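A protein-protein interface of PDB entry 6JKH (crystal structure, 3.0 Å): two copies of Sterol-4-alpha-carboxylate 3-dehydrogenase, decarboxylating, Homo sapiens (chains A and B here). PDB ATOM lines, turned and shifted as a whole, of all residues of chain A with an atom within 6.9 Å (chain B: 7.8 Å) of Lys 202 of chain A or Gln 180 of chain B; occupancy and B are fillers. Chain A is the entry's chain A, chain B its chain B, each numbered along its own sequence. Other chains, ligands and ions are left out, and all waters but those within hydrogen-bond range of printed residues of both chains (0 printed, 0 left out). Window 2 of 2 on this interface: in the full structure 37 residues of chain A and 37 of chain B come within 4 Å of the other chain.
The backbone NH (N) of Gly 199 of chain A is in hydrogen-bond range of the backbone carbonyl oxygen (O) of Val 182 of chain B, at 2.6 Å.
N of Gly 201 of chain A is in hydrogen-bond range of O of Gln 180 of chain B, at 3.0 Å.
Among the printed residues, merely in contact across the chains: Lys 202 of chain A with Gln 180 of chain B (3.0 Å), Gly 201 of chain A with Val 182 of chain B (3.3 Å), Gly 199 of chain A with Leu 181 of chain B (3.6 Å), Asn 200 of chain A with Leu 181 of chain B (3.8 Å) and Asn 200 of chain A with Gln 180 of chain B (3.9 Å).
Of chain B, only Gln 180 (3.0 Å) comes within 4 Å of Lys 202 of chain A.
Gln 180 of chain B touches just these residues of chain A: Asn 200, Gly 201 and Lys 202.
Of chain B, only Gln 180 (3.0 Å) and Val 182 (3.3 Å) come within 4 Å of Gly 201 of chain A.
Printed residues of chain A within 4 Å of Val 182 of chain B: Gly 199 and Gly 201.
Of the printed residues of chain A, Leu 181 of chain B touches Gly 199 and Asn 200.
Of the printed residues of chain B, Asn 200 of chain A touches Gln 180 and Leu 181.
Printed residues of chain B within 4 Å of Gly 199 of chain A: Leu 181 and Val 182.
The nearest residue of chain B that does not touch Lys 202 of chain A is Val 182 of chain B (6.0 Å).
The nearest printed residue of chain B that does not touch Gly 199 of chain A is Pro 183 of chain B (4.5 Å).
Of the 8 printed residues of chain A, 4 touch a printed residue of chain B.
Hydrophobic or aromatic side chains of chain B that line the printed part of chain A: Leu 181 and Val 182.
Among the printed residues, 7 pairs touch across the chains.
No position is printed for both chains.
Of the 7 pairs that touch across the chains among the printed residues, none has its exchanged pair printed and touching as well.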
ATOM      1  N   GLY A 199      18.220  -3.203  -3.658  1.00  0.00           N
ATOM      2  CA  GLY A 199      18.828  -4.351  -2.964  1.00  0.00           C
ATOM      3  C   GLY A 199      19.738  -3.860  -1.856  1.00  0.00           C
ATOM      4  O   GLY A 199      19.999  -2.630  -1.810  1.00  0.00           O
ATOM      5  N   ASN A 200      20.298  -4.785  -1.081  1.00  0.00           N
ATOM      6  CA  ASN A 200      21.274  -4.440  -0.017  1.00  0.00           C
ATOM      7  C   ASN A 200      22.609  -5.076  -0.387  1.00  0.00           C
ATOM      8  O   ASN A 200      22.762  -6.265  -0.147  1.00  0.00           O
ATOM      9  CB  ASN A 200      20.809  -4.888   1.366  1.00  0.00           C
ATOM     10  CG  ASN A 200      19.497  -4.243   1.752  1.00  0.00           C
ATOM     11  OD1 ASN A 200      18.704  -3.887   0.883  1.00  0.00           O
ATOM     12  ND2 ASN A 200      19.263  -4.082   3.043  1.00  0.00           N
ATOM     13  N   GLY A 201      23.552  -4.271  -0.883  1.00  0.00           N
ATOM     14  CA  GLY A 201      24.896  -4.673  -1.350  1.00  0.00           C
ATOM     15  C   GLY A 201      25.607  -5.741  -0.539  1.00  0.00           C
ATOM     16  O   GLY A 201      26.241  -6.588  -1.156  1.00  0.00           O
ATOM     17  N   LYS A 202      25.535  -5.695   0.794  1.00  0.00           N
ATOM     18  CA  LYS A 202      26.194  -6.690   1.679  1.00  0.00           C
ATOM     19  C   LYS A 202      25.796  -8.121   1.309  1.00  0.00           C
ATOM     20  O   LYS A 202      26.692  -8.978   1.290  1.00  0.00           O
ATOM     21  CB  LYS A 202      25.890  -6.388   3.145  1.00  0.00           C
ATOM     22  CG  LYS A 202      27.046  -5.750   3.897  1.00  0.00           C
ATOM     23  CD  LYS A 202      28.340  -5.753   3.114  1.00  0.00           C
ATOM     24  CE  LYS A 202      29.571  -5.563   3.974  1.00  0.00           C
ATOM     25  NZ  LYS A 202      30.297  -6.833   4.204  1.00  0.00           N
ATOM     26  N   ASN A 203      24.572  -8.341   0.837  1.00  0.00           N
ATOM     27  CA  ASN A 203      24.182  -9.721   0.448  1.00  0.00           C
ATOM     28  C   ASN A 203      24.496 -10.011  -1.027  1.00  0.00           C
ATOM     29  O   ASN A 203      24.322 -11.150  -1.427  1.00  0.00           O
ATOM     30  CB  ASN A 203      22.701  -9.981   0.733  1.00  0.00           C
ATOM     31  CG  ASN A 203      22.410 -11.419   1.115  1.00  0.00           C
ATOM     32  OD1 ASN A 203      21.569 -12.076   0.501  1.00  0.00           O
ATOM     33  ND2 ASN A 203      23.096 -11.919   2.133  1.00  0.00           N
ATOM     34  N   LEU A 204      24.998  -9.050  -1.796  1.00  0.00           N
ATOM     35  CA  LEU A 204      25.147  -9.274  -3.258  1.00  0.00           C
ATOM     36  C   LEU A 204      26.561  -9.546  -3.754  1.00  0.00           C
ATOM     37  O   LEU A 204      26.690  -9.867  -4.935  1.00  0.00           O
ATOM     38  CB  LEU A 204      24.712  -7.979  -3.945  1.00  0.00           C
ATOM     39  CG  LEU A 204      23.219  -7.810  -4.178  1.00  0.00           C
ATOM     40  CD1 LEU A 204      22.839  -8.318  -5.552  1.00  0.00           C
ATOM     41  CD2 LEU A 204      22.430  -8.528  -3.106  1.00  0.00           C
ATOM     42  N   VAL A 205      27.589  -9.353  -2.951  1.00  0.00           N
ATOM     43  CA  VAL A 205      28.942  -9.392  -3.586  1.00  0.00           C
ATOM     44  C   VAL A 205      29.407 -10.758  -4.116  1.00  0.00           C
ATOM     45  O   VAL A 205      29.874 -10.802  -5.258  1.00  0.00           O
ATOM     46  CB  VAL A 205      29.979  -8.718  -2.675  1.00  0.00           C
ATOM     47  CG1 VAL A 205      30.329  -7.336  -3.200  1.00  0.00           C
ATOM     48  CG2 VAL A 205      29.465  -8.625  -1.248  1.00  0.00           C
ATOM     49  N   ASP A 206      29.223 -11.818  -3.336  1.00  0.00           N
ATOM     50  CA  ASP A 206      29.749 -13.181  -3.601  1.00  0.00           C
ATOM     51  C   ASP A 206      28.795 -13.932  -4.542  1.00  0.00           C
ATOM     52  O   ASP A 206      29.050 -15.120  -4.808  1.00  0.00           O
ATOM     53  CB  ASP A 206      29.969 -13.917  -2.275  1.00  0.00           C
ATOM     54  CG  ASP A 206      28.766 -13.921  -1.342  1.00  0.00           C
ATOM     55  OD1 ASP A 206      27.772 -13.221  -1.648  1.00  0.00           O
ATOM     56  OD2 ASP A 206      28.841 -14.602  -0.304  1.00  0.00           O
ATOM     57  N   PHE B 120      17.715   7.799  -6.300  1.00  0.00           N
ATOM     58  CA  PHE B 120      17.219   7.760  -4.900  1.00  0.00           C
ATOM     59  C   PHE B 120      16.646   9.095  -4.417  1.00  0.00           C
ATOM     60  O   PHE B 120      16.213   9.141  -3.282  1.00  0.00           O
ATOM     61  CB  PHE B 120      18.381   7.437  -3.967  1.00  0.00           C
ATOM     62  CG  PHE B 120      18.837   6.012  -4.045  1.00  0.00           C
ATOM     63  CD1 PHE B 120      18.122   5.015  -3.423  1.00  0.00           C
ATOM     64  CD2 PHE B 120      19.960   5.663  -4.757  1.00  0.00           C
ATOM     65  CE1 PHE B 120      18.529   3.700  -3.506  1.00  0.00           C
ATOM     66  CE2 PHE B 120      20.364   4.348  -4.841  1.00  0.00           C
ATOM     67  CZ  PHE B 120      19.648   3.373  -4.211  1.00  0.00           C
ATOM     68  N   ASP B 140      23.617  10.941   0.234  1.00  0.00           N
ATOM     69  CA  ASP B 140      24.669  11.863   0.747  1.00  0.00           C
ATOM     70  C   ASP B 140      24.425  13.280   0.254  1.00  0.00           C
ATOM     71  O   ASP B 140      23.702  13.458  -0.746  1.00  0.00           O
ATOM     72  CB  ASP B 140      26.071  11.521   0.234  1.00  0.00           C
ATOM     73  CG  ASP B 140      26.566  10.129   0.564  1.00  0.00           C
ATOM     74  OD1 ASP B 140      25.762   9.302   1.053  1.00  0.00           O
ATOM     75  OD2 ASP B 140      27.760   9.884   0.314  1.00  0.00           O
ATOM     76  N   HIS B 171      27.008   2.668 -11.558  1.00  0.00           N
ATOM     77  CA  HIS B 171      26.803   2.209 -10.161  1.00  0.00           C
ATOM     78  C   HIS B 171      28.103   2.350  -9.358  1.00  0.00           C
ATOM     79  O   HIS B 171      28.939   3.193  -9.736  1.00  0.00           O
ATOM     80  CB  HIS B 171      26.283   0.765 -10.173  1.00  0.00           C
ATOM     81  CG  HIS B 171      26.635  -0.036  -8.962  1.00  0.00           C
ATOM     82  ND1 HIS B 171      27.525  -1.101  -9.010  1.00  0.00           N
ATOM     83  CD2 HIS B 171      26.210   0.047  -7.682  1.00  0.00           C
ATOM     84  CE1 HIS B 171      27.627  -1.641  -7.813  1.00  0.00           C
ATOM     85  NE2 HIS B 171      26.833  -0.954  -6.980  1.00  0.00           N
ATOM     86  N   GLN B 180      25.448   1.740   0.799  1.00  0.00           N
ATOM     87  CA  GLN B 180      25.367   0.253   0.849  1.00  0.00           C
ATOM     88  C   GLN B 180      24.041  -0.261   0.263  1.00  0.00           C
ATOM     89  O   GLN B 180      23.981  -1.438  -0.144  1.00  0.00           O
ATOM     90  CB  GLN B 180      25.514  -0.222   2.293  1.00  0.00           C
ATOM     91  CG  GLN B 180      25.631  -1.734   2.404  1.00  0.00           C
ATOM     92  CD  GLN B 180      26.711  -2.158   3.367  1.00  0.00           C
ATOM     93  OE1 GLN B 180      26.453  -2.874   4.335  1.00  0.00           O
ATOM     94  NE2 GLN B 180      27.933  -1.715   3.095  1.00  0.00           N
ATOM     95  N   LEU B 181      23.008   0.583   0.268  1.00  0.00           N
ATOM     96  CA  LEU B 181      21.656   0.334  -0.294  1.00  0.00           C
ATOM     97  C   LEU B 181      21.679   0.578  -1.809  1.00  0.00           C
ATOM     98  O   LEU B 181      21.619   1.731  -2.215  1.00  0.00           O
ATOM     99  CB  LEU B 181      20.716   1.308   0.423  1.00  0.00           C
ATOM    100  CG  LEU B 181      19.223   1.090   0.220  1.00  0.00           C
ATOM    101  CD1 LEU B 181      18.729  -0.080   1.048  1.00  0.00           C
ATOM    102  CD2 LEU B 181      18.452   2.350   0.574  1.00  0.00           C
ATOM    103  N   VAL B 182      21.727  -0.482  -2.609  1.00  0.00           N
ATOM    104  CA  VAL B 182      22.065  -0.441  -4.064  1.00  0.00           C
ATOM    105  C   VAL B 182      20.803  -0.736  -4.869  1.00  0.00           C
ATOM    106  O   VAL B 182      20.024  -1.594  -4.477  1.00  0.00           O
ATOM    107  CB  VAL B 182      23.174  -1.464  -4.385  1.00  0.00           C
ATOM    108  CG1 VAL B 182      22.893  -2.826  -3.773  1.00  0.00           C
ATOM    109  CG2 VAL B 182      23.426  -1.619  -5.880  1.00  0.00           C
ATOM    110  N   PRO B 183      20.577  -0.068  -6.026  1.00  0.00           N
ATOM    111  CA  PRO B 183      19.462  -0.407  -6.919  1.00  0.00           C
ATOM    112  C   PRO B 183      19.751  -1.583  -7.867  1.00  0.00           C
ATOM    113  O   PRO B 183      20.785  -1.597  -8.490  1.00  0.00           O
ATOM    114  CB  PRO B 183      19.295   0.872  -7.751  1.00  0.00           C
ATOM    115  CG  PRO B 183      20.703   1.441  -7.836  1.00  0.00           C
ATOM    116  CD  PRO B 183      21.373   1.064  -6.528  1.00  0.00           C
